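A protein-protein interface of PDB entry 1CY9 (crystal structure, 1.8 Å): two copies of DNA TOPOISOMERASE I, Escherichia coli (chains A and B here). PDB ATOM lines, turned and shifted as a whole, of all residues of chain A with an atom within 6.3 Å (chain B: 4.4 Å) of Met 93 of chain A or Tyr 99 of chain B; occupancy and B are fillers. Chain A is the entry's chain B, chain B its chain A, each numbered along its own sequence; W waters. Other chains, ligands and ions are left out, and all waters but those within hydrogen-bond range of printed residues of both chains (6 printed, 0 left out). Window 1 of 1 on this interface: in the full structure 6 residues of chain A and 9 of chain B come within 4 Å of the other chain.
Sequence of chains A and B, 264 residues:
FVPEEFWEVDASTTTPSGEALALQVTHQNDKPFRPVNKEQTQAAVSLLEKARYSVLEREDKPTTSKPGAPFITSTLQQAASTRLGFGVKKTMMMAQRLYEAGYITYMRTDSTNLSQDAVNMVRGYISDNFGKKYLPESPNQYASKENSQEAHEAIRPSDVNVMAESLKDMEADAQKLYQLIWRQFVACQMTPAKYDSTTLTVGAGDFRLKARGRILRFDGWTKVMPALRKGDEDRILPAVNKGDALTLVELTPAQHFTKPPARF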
ATOM      1  N   VAL A  88     -35.431  27.138  23.759  1.00  0.00           N
ATOM      2  CA  VAL A  88     -35.487  28.110  22.668  1.00  0.00           C
ATOM      3  C   VAL A  88     -34.366  29.141  22.672  1.00  0.00           C
ATOM      4  O   VAL A  88     -33.729  29.403  21.650  1.00  0.00           O
ATOM      5  CB  VAL A  88     -36.829  28.858  22.684  1.00  0.00           C
ATOM      6  CG1 VAL A  88     -36.753  30.105  21.815  1.00  0.00           C
ATOM      7  CG2 VAL A  88     -37.928  27.926  22.194  1.00  0.00           C
ATOM      8  N   LYS A  89     -34.148  29.735  23.834  1.00  0.00           N
ATOM      9  CA  LYS A  89     -33.135  30.756  24.018  1.00  0.00           C
ATOM     10  C   LYS A  89     -31.753  30.214  23.648  1.00  0.00           C
ATOM     11  O   LYS A  89     -31.006  30.840  22.889  1.00  0.00           O
ATOM     12  CB  LYS A  89     -33.155  31.199  25.485  1.00  0.00           C
ATOM     13  CG  LYS A  89     -34.560  31.172  26.150  1.00  0.00           C
ATOM     14  CD  LYS A  89     -35.256  29.764  26.219  1.00  0.00           C
ATOM     15  CE  LYS A  89     -34.443  28.724  27.003  1.00  0.00           C
ATOM     16  NZ  LYS A  89     -33.169  28.263  26.346  1.00  0.00           N
ATOM     17  N   LYS A  90     -31.417  29.048  24.192  1.00  0.00           N
ATOM     18  CA  LYS A  90     -30.125  28.412  23.916  1.00  0.00           C
ATOM     19  C   LYS A  90     -29.961  28.110  22.429  1.00  0.00           C
ATOM     20  O   LYS A  90     -28.908  28.356  21.832  1.00  0.00           O
ATOM     21  CB  LYS A  90     -29.993  27.113  24.734  1.00  0.00           C
ATOM     22  CG  LYS A  90     -28.717  26.306  24.415  1.00  0.00           C
ATOM     23  CD  LYS A  90     -28.530  25.107  25.355  1.00  0.00           C
ATOM     24  CE  LYS A  90     -27.345  24.262  24.894  1.00  0.00           C
ATOM     25  NZ  LYS A  90     -27.114  23.085  25.763  1.00  0.00           N
ATOM     26  N   THR A  91     -31.006  27.561  21.825  1.00  0.00           N
ATOM     27  CA  THR A  91     -30.949  27.240  20.413  1.00  0.00           C
ATOM     28  C   THR A  91     -30.678  28.482  19.593  1.00  0.00           C
ATOM     29  O   THR A  91     -29.845  28.466  18.707  1.00  0.00           O
ATOM     30  CB  THR A  91     -32.270  26.607  19.925  1.00  0.00           C
ATOM     31  OG1 THR A  91     -32.409  25.315  20.524  1.00  0.00           O
ATOM     32  CG2 THR A  91     -32.268  26.456  18.398  1.00  0.00           C
ATOM     33  N   MET A  92     -31.381  29.565  19.899  1.00  0.00           N
ATOM     34  CA  MET A  92     -31.188  30.777  19.127  1.00  0.00           C
ATOM     35  C   MET A  92     -29.820  31.411  19.339  1.00  0.00           C
ATOM     36  O   MET A  92     -29.290  32.046  18.437  1.00  0.00           O
ATOM     37  CB  MET A  92     -32.310  31.773  19.412  1.00  0.00           C
ATOM     38  CG  MET A  92     -33.666  31.309  18.888  1.00  0.00           C
ATOM     39  SD  MET A  92     -33.620  30.616  17.217  1.00  0.00           S
ATOM     40  CE  MET A  92     -33.386  32.113  16.254  1.00  0.00           C
ATOM     41  N   MET A  93     -29.240  31.235  20.522  1.00  0.00           N
ATOM     42  CA  MET A  93     -27.919  31.791  20.793  1.00  0.00           C
ATOM     43  C   MET A  93     -26.890  31.012  19.962  1.00  0.00           C
ATOM     44  O   MET A  93     -25.980  31.589  19.365  1.00  0.00           O
ATOM     45  CB  MET A  93     -27.609  31.671  22.293  1.00  0.00           C
ATOM     46  CG  MET A  93     -26.598  32.659  22.820  1.00  0.00           C
ATOM     47  SD  MET A  93     -26.570  32.681  24.654  1.00  0.00           S
ATOM     48  CE  MET A  93     -28.216  33.012  24.988  1.00  0.00           C
ATOM     49  N   MET A  94     -27.040  29.691  19.917  1.00  0.00           N
ATOM     50  CA  MET A  94     -26.123  28.874  19.142  1.00  0.00           C
ATOM     51  C   MET A  94     -26.305  29.091  17.646  1.00  0.00           C
ATOM     52  O   MET A  94     -25.329  29.135  16.894  1.00  0.00           O
ATOM     53  CB  MET A  94     -26.312  27.387  19.466  1.00  0.00           C
ATOM     54  CG  MET A  94     -25.747  26.979  20.818  1.00  0.00           C
ATOM     55  SD  MET A  94     -25.852  25.175  21.023  1.00  0.00           S
ATOM     56  CE  MET A  94     -27.549  24.981  21.150  1.00  0.00           C
ATOM     57  N   ALA A  95     -27.552  29.193  17.207  1.00  0.00           N
ATOM     58  CA  ALA A  95     -27.802  29.406  15.785  1.00  0.00           C
ATOM     59  C   ALA A  95     -27.176  30.743  15.383  1.00  0.00           C
ATOM     60  O   ALA A  95     -26.591  30.858  14.312  1.00  0.00           O
ATOM     61  CB  ALA A  95     -29.294  29.409  15.511  1.00  0.00           C
ATOM     62  N   GLN A  96     -27.282  31.753  16.244  1.00  0.00           N
ATOM     63  CA  GLN A  96     -26.701  33.054  15.915  1.00  0.00           C
ATOM     64  C   GLN A  96     -25.187  32.942  15.753  1.00  0.00           C
ATOM     65  O   GLN A  96     -24.612  33.523  14.833  1.00  0.00           O
ATOM     66  CB  GLN A  96     -27.035  34.103  16.986  1.00  0.00           C
ATOM     67  CG  GLN A  96     -26.654  35.516  16.564  1.00  0.00           C
ATOM     68  CD  GLN A  96     -26.991  36.562  17.607  1.00  0.00           C
ATOM     69  OE1 GLN A  96     -28.077  36.547  18.190  1.00  0.00           O
ATOM     70  NE2 GLN A  96     -26.068  37.493  17.831  1.00  0.00           N
ATOM     71  N   ARG A  97     -24.534  32.172  16.620  1.00  0.00           N
ATOM     72  CA  ARG A  97     -23.094  32.003  16.521  1.00  0.00           C
ATOM     73  C   ARG A  97     -22.694  31.243  15.254  1.00  0.00           C
ATOM     74  O   ARG A  97     -21.683  31.559  14.636  1.00  0.00           O
ATOM     75  CB  ARG A  97     -22.555  31.291  17.769  1.00  0.00           C
ATOM     76  CG  ARG A  97     -22.532  32.201  19.006  1.00  0.00           C
ATOM     77  CD  ARG A  97     -22.242  31.406  20.265  1.00  0.00           C
ATOM     78  NE  ARG A  97     -21.033  30.611  20.091  1.00  0.00           N
ATOM     79  CZ  ARG A  97     -20.893  29.365  20.526  1.00  0.00           C
ATOM     80  NH1 ARG A  97     -19.753  28.716  20.319  1.00  0.00           N
ATOM     81  NH2 ARG A  97     -21.896  28.764  21.159  1.00  0.00           N
ATOM     82  N   LEU A  98     -23.491  30.256  14.850  1.00  0.00           N
ATOM     83  CA  LEU A  98     -23.165  29.487  13.647  1.00  0.00           C
ATOM     84  C   LEU A  98     -23.276  30.395  12.412  1.00  0.00           C
ATOM     85  O   LEU A  98     -22.464  30.301  11.490  1.00  0.00           O
ATOM     86  CB  LEU A  98     -24.117  28.296  13.501  1.00  0.00           C
ATOM     87  CG  LEU A  98     -23.922  27.117  14.465  1.00  0.00           C
ATOM     88  CD1 LEU A  98     -25.108  26.172  14.326  1.00  0.00           C
ATOM     89  CD2 LEU A  98     -22.610  26.390  14.169  1.00  0.00           C
ATOM     90  N   GLU A 171     -18.288  24.189  20.166  1.00  0.00           N
ATOM     91  CA  GLU A 171     -18.406  23.154  21.188  1.00  0.00           C
ATOM     92  C   GLU A 171     -19.357  22.064  20.685  1.00  0.00           C
ATOM     93  O   GLU A 171     -20.077  22.256  19.696  1.00  0.00           O
ATOM     94  CB  GLU A 171     -18.915  23.740  22.518  1.00  0.00           C
ATOM     95  CG  GLU A 171     -20.367  24.202  22.533  1.00  0.00           C
ATOM     96  CD  GLU A 171     -20.597  25.561  21.889  1.00  0.00           C
ATOM     97  OE1 GLU A 171     -19.641  26.156  21.340  1.00  0.00           O
ATOM     98  OE2 GLU A 171     -21.752  26.036  21.935  1.00  0.00           O
ATOM     99  N   ASP A 173     -22.326  20.825  21.578  1.00  0.00           N
ATOM    100  CA  ASP A 173     -23.742  21.108  21.332  1.00  0.00           C
ATOM    101  C   ASP A 173     -23.969  21.962  20.077  1.00  0.00           C
ATOM    102  O   ASP A 173     -25.001  21.829  19.416  1.00  0.00           O
ATOM    103  CB  ASP A 173     -24.393  21.788  22.543  1.00  0.00           C
ATOM    104  CG  ASP A 173     -24.675  20.818  23.684  1.00  0.00           C
ATOM    105  OD1 ASP A 173     -24.733  19.591  23.435  1.00  0.00           O
ATOM    106  OD2 ASP A 173     -24.858  21.288  24.830  1.00  0.00           O
ATOM    107  N   ALA B  95     -23.803  28.134  36.409  1.00  0.00           N
ATOM    108  CA  ALA B  95     -23.560  28.878  35.176  1.00  0.00           C
ATOM    109  C   ALA B  95     -24.187  28.123  34.000  1.00  0.00           C
ATOM    110  O   ALA B  95     -24.781  28.723  33.103  1.00  0.00           O
ATOM    111  CB  ALA B  95     -22.062  29.052  34.961  1.00  0.00           C
ATOM    112  N   GLN B  96     -24.075  26.796  34.003  1.00  0.00           N
ATOM    113  CA  GLN B  96     -24.669  26.031  32.918  1.00  0.00           C
ATOM    114  C   GLN B  96     -26.181  26.208  32.902  1.00  0.00           C
ATOM    115  O   GLN B  96     -26.771  26.306  31.836  1.00  0.00           O
ATOM    116  CB  GLN B  96     -24.304  24.543  33.004  1.00  0.00           C
ATOM    117  CG  GLN B  96     -24.816  23.751  31.792  1.00  0.00           C
ATOM    118  CD  GLN B  96     -24.309  22.319  31.753  1.00  0.00           C
ATOM    119  OE1 GLN B  96     -23.125  22.062  31.973  1.00  0.00           O
ATOM    120  NE2 GLN B  96     -25.197  21.387  31.453  1.00  0.00           N
ATOM    121  N   ARG B  97     -26.818  26.261  34.072  1.00  0.00           N
ATOM    122  CA  ARG B  97     -28.254  26.461  34.108  1.00  0.00           C
ATOM    123  C   ARG B  97     -28.647  27.865  33.625  1.00  0.00           C
ATOM    124  O   ARG B  97     -29.663  28.028  32.945  1.00  0.00           O
ATOM    125  CB  ARG B  97     -28.790  26.210  35.510  1.00  0.00           C
ATOM    126  CG  ARG B  97     -28.800  24.721  35.861  1.00  0.00           C
ATOM    127  CD  ARG B  97     -29.096  24.545  37.324  1.00  0.00           C
ATOM    128  NE  ARG B  97     -30.292  25.296  37.670  1.00  0.00           N
ATOM    129  CZ  ARG B  97     -30.450  25.952  38.808  1.00  0.00           C
ATOM    130  NH1 ARG B  97     -31.577  26.610  39.033  1.00  0.00           N
ATOM    131  NH2 ARG B  97     -29.476  25.961  39.712  1.00  0.00           N
ATOM    132  N   LEU B  98     -27.852  28.874  33.972  1.00  0.00           N
ATOM    133  CA  LEU B  98     -28.144  30.234  33.519  1.00  0.00           C
ATOM    134  C   LEU B  98     -28.040  30.320  31.990  1.00  0.00           C
ATOM    135  O   LEU B  98     -28.841  30.997  31.341  1.00  0.00           O
ATOM    136  CB  LEU B  98     -27.178  31.234  34.162  1.00  0.00           C
ATOM    137  CG  LEU B  98     -27.367  31.555  35.648  1.00  0.00           C
ATOM    138  CD1 LEU B  98     -26.195  32.415  36.112  1.00  0.00           C
ATOM    139  CD2 LEU B  98     -28.698  32.283  35.890  1.00  0.00           C
ATOM    140  N   TYR B  99     -27.059  29.626  31.433  1.00  0.00           N
ATOM    141  CA  TYR B  99     -26.833  29.585  29.996  1.00  0.00           C
ATOM    142  C   TYR B  99     -27.970  28.818  29.300  1.00  0.00           C
ATOM    143  O   TYR B  99     -28.514  29.264  28.289  1.00  0.00           O
ATOM    144  CB  TYR B  99     -25.492  28.899  29.703  1.00  0.00           C
ATOM    145  CG  TYR B  99     -25.270  28.569  28.237  1.00  0.00           C
ATOM    146  CD1 TYR B  99     -25.218  29.580  27.278  1.00  0.00           C
ATOM    147  CD2 TYR B  99     -25.142  27.240  27.808  1.00  0.00           C
ATOM    148  CE1 TYR B  99     -25.046  29.281  25.922  1.00  0.00           C
ATOM    149  CE2 TYR B  99     -24.968  26.925  26.461  1.00  0.00           C
ATOM    150  CZ  TYR B  99     -24.922  27.953  25.524  1.00  0.00           C
ATOM    151  OH  TYR B  99     -24.748  27.672  24.194  1.00  0.00           O
ATOM    152  N   GLU B 100     -28.346  27.671  29.854  1.00  0.00           N
ATOM    153  CA  GLU B 100     -29.398  26.883  29.226  1.00  0.00           C
ATOM    154  C   GLU B 100     -30.750  27.588  29.241  1.00  0.00           C
ATOM    155  O   GLU B 100     -31.607  27.315  28.398  1.00  0.00           O
ATOM    156  CB  GLU B 100     -29.467  25.499  29.881  1.00  0.00           C
ATOM    157  CG  GLU B 100     -28.167  24.720  29.684  1.00  0.00           C
ATOM    158  CD  GLU B 100     -28.174  23.361  30.355  1.00  0.00           C
ATOM    159  OE1 GLU B 100     -28.945  23.173  31.314  1.00  0.00           O
ATOM    160  OE2 GLU B 100     -27.390  22.485  29.931  1.00  0.00           O
ATOM    161  N   ALA B 101     -30.929  28.508  30.185  1.00  0.00           N
ATOM    162  CA  ALA B 101     -32.152  29.279  30.292  1.00  0.00           C
ATOM    163  C   ALA B 101     -32.046  30.521  29.397  1.00  0.00           C
ATOM    164  O   ALA B 101     -33.018  31.250  29.227  1.00  0.00           O
ATOM    165  CB  ALA B 101     -32.381  29.687  31.723  1.00  0.00           C
ATOM    166  N   GLY B 102     -30.855  30.749  28.849  1.00  0.00           N
ATOM    167  CA  GLY B 102     -30.628  31.876  27.955  1.00  0.00           C
ATOM    168  C   GLY B 102     -30.264  33.204  28.599  1.00  0.00           C
ATOM    169  O   GLY B 102     -30.251  34.239  27.920  1.00  0.00           O
ATOM    170  N   ILE B 104     -27.256  34.010  30.170  1.00  0.00           N
ATOM    171  CA  ILE B 104     -25.867  34.404  29.946  1.00  0.00           C
ATOM    172  C   ILE B 104     -25.318  33.675  28.725  1.00  0.00           C
ATOM    173  O   ILE B 104     -25.944  32.753  28.222  1.00  0.00           O
ATOM    174  CB  ILE B 104     -24.945  34.076  31.152  1.00  0.00           C
ATOM    175  CG1 ILE B 104     -24.887  32.552  31.377  1.00  0.00           C
ATOM    176  CG2 ILE B 104     -25.459  34.807  32.413  1.00  0.00           C
ATOM    177  CD1 ILE B 104     -23.834  32.107  32.395  1.00  0.00           C
ATOM    178  N   THR B 105     -24.158  34.109  28.250  1.00  0.00           N
ATOM    179  CA  THR B 105     -23.520  33.494  27.096  1.00  0.00           C
ATOM    180  C   THR B 105     -22.821  32.200  27.531  1.00  0.00           C
ATOM    181  O   THR B 105     -22.741  31.895  28.728  1.00  0.00           O
ATOM    182  CB  THR B 105     -22.514  34.463  26.447  1.00  0.00           C
ATOM    183  OG1 THR B 105     -21.585  34.919  27.432  1.00  0.00           O
ATOM    184  CG2 THR B 105     -23.251  35.684  25.873  1.00  0.00           C
ATOM    185  N   TYR B 106     -22.335  31.436  26.557  1.00  0.00           N
ATOM    186  CA  TYR B 106     -21.671  30.162  26.825  1.00  0.00           C
ATOM    187  C   TYR B 106     -20.605  30.300  27.911  1.00  0.00           C
ATOM    188  O   TYR B 106     -19.738  31.169  27.835  1.00  0.00           O
ATOM    189  CB  TYR B 106     -21.088  29.606  25.527  1.00  0.00           C
ATOM    190  CG  TYR B 106     -20.542  28.207  25.653  1.00  0.00           C
ATOM    191  CD1 TYR B 106     -21.346  27.162  26.111  1.00  0.00           C
ATOM    192  CD2 TYR B 106     -19.225  27.922  25.307  1.00  0.00           C
ATOM    193  CE1 TYR B 106     -20.844  25.864  26.219  1.00  0.00           C
ATOM    194  CE2 TYR B 106     -18.716  26.630  25.412  1.00  0.00           C
ATOM    195  CZ  TYR B 106     -19.531  25.609  25.867  1.00  0.00           C
ATOM    196  OH  TYR B 106     -19.031  24.330  25.970  1.00  0.00           O
ATOM    197  N   MET B 107     -20.669  29.418  28.911  1.00  0.00           N
ATOM    198  CA  MET B 107     -19.790  29.492  30.072  1.00  0.00           C
ATOM    199  C   MET B 107     -18.419  28.828  30.030  1.00  0.00           C
ATOM    200  O   MET B 107     -17.712  28.829  31.035  1.00  0.00           O
ATOM    201  CB  MET B 107     -20.546  28.996  31.318  1.00  0.00           C
ATOM    202  CG  MET B 107     -20.921  27.509  31.303  1.00  0.00           C
ATOM    203  SD  MET B 107     -22.277  27.068  30.199  1.00  0.00           S
ATOM    204  CE  MET B 107     -21.858  25.362  29.880  1.00  0.00           C
ATOM    205  N   SER B 158     -27.017  37.985  28.482  1.00  0.00           N
ATOM    206  CA  SER B 158     -27.514  38.058  27.114  1.00  0.00           C
ATOM    207  C   SER B 158     -28.231  39.388  26.881  1.00  0.00           C
ATOM    208  O   SER B 158     -28.169  39.938  25.787  1.00  0.00           O
ATOM    209  CB  SER B 158     -28.475  36.898  26.844  1.00  0.00           C
ATOM    210  OG  SER B 158     -27.757  35.682  26.772  1.00  0.00           O
HETATM  211  O   HOH W   1     -23.163  32.079  23.873  1.00  0.00           O
HETATM  212  O   HOH W   2     -24.132  29.811  22.434  1.00  0.00           O
HETATM  213  O   HOH W   3     -23.672  25.426  23.522  1.00  0.00           O
HETATM  214  O   HOH W   4     -26.761  36.025  23.897  1.00  0.00           O
HETATM  215  O   HOH W   5     -25.484  23.786  28.067  1.00  0.00           O
HETATM  216  O   HOH W   6     -28.215  30.208  25.757  1.00  0.00           O
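4 positions are printed for both chains. Of the 11 pairs that touch across the chains among the printed residues, none has its exchanged pair printed and touching as well.
OE2 of Glu 100 of chain B is in hydrogen-bond range of NE2 of Gln 96 of chain B. OG of Ser 158 of chain B is in hydrogen-bond range of O of Gly 102 of chain B (3.1 Å). NZ of Lys 90 of chain A is in salt-bridge range of OD2 of Asp 173 of chain A. The guanidinium group (NH1) of Arg 97 of chain A is in salt-bridge range of the side-chain carboxylate (OE1) of Glu 171 of chain A.
The backbone carbonyl oxygen of Glu 100 of chain B lies within hydrogen-bond range of the side-chain amino group of Lys 89 of chain A, 2.7 Å away. SD of Met 93 of chain A lies close to O of Ile 104 of chain B (3.6 Å).
Water W3 lies within hydrogen-bond range of OE2 of Glu 171 of chain A (2.6 Å), OH of Tyr 99 of chain B (2.6 Å) and SD of Met 94 of chain A (3.3 Å). Water W6 bridges O of Tyr 99 of chain B (2.7 Å) and SD of Met 93 of chain A (3.2 Å). Water W2 bridges the guanidinium group (NH2) of Arg 97 of chain A (2.8 Å) and the side-chain hydroxyl (OH) of Tyr 99 of chain B (2.8 Å). Water W1 bridges N of Tyr 106 of chain B and SD of Met 93 of chain A. Water W5 lies within hydrogen-bond range of NZ of Lys 90 of chain A (2.9 Å) and OE2 of Glu 100 of chain B (3.0 Å). Water W4 bridges the side-chain hydroxyl of Ser 158 of chain B (3.1 Å) and the side-chain sulfur of Met 93 of chain A (3.4 Å).
Of the 13 printed residues of chain B, 8 touch a printed residue of chain A. Hydrophobic or aromatic side chains of chain B that line the printed part of chain A: Tyr 99 and Tyr 106. Of the 13 printed residues of chain A, 5 touch a printed residue of chain B. Hydrophobic or aromatic side chains of chain A that line the printed part of chain B: Met 93 and Met 94. Among the printed residues, no Asp or Glu carboxylate lies within 4 Å of a Lys or Arg side-chain nitrogen of the other chain.
Printed residues of chain B within 4 Å of Met 93 of chain A: Tyr 99 (3.9 Å), Gly 102 (3.8 Å), Ile 104 (3.6 Å), Thr 105 (3.99 Å) and Ser 158 (3.2 Å). Printed residues of chain B within 4 Å of Glu 171 of chain A: Tyr 106. Tyr 99 of chain B touches three residues of chain A. Of the printed residues of chain A, Gly 102 of chain B touches Lys 89 (3.6 Å) and Met 93 (3.8 Å). The nearest printed residue of chain B that does not touch Met 93 of chain A is Tyr 106 of chain B (4.8 Å). The nearest residue of chain A that does not touch Tyr 99 of chain B is Glu 171 of chain A (4.1 Å).
Ala 101 of chain B touches Lys 89 of chain A (O to CG, 3.4 Å). CB of Lys 89 of chain A touches CA of Gly 102 of chain B, at 3.6 Å. Lys 90 of chain A touches Tyr 99 of chain B (CE to CE2, 3.9 Å). CE1 of Tyr 99 of chain B touches SD of Met 93 of chain A, at 3.9 Å. O of Gly 102 of chain B touches CE of Met 93 of chain A, 3.8 Å away. Met 93 of chain A touches Thr 105 of chain B (SD to CA, 3.99 Å). Ser 158 of chain B touches Met 93 of chain A (OG to CE, 3.2 Å). OH of Tyr 99 of chain B touches CG of Met 94 of chain A, at 3.6 Å. CB of Glu 171 of chain A touches OH of Tyr 106 of chain B, at 3.5 Å.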
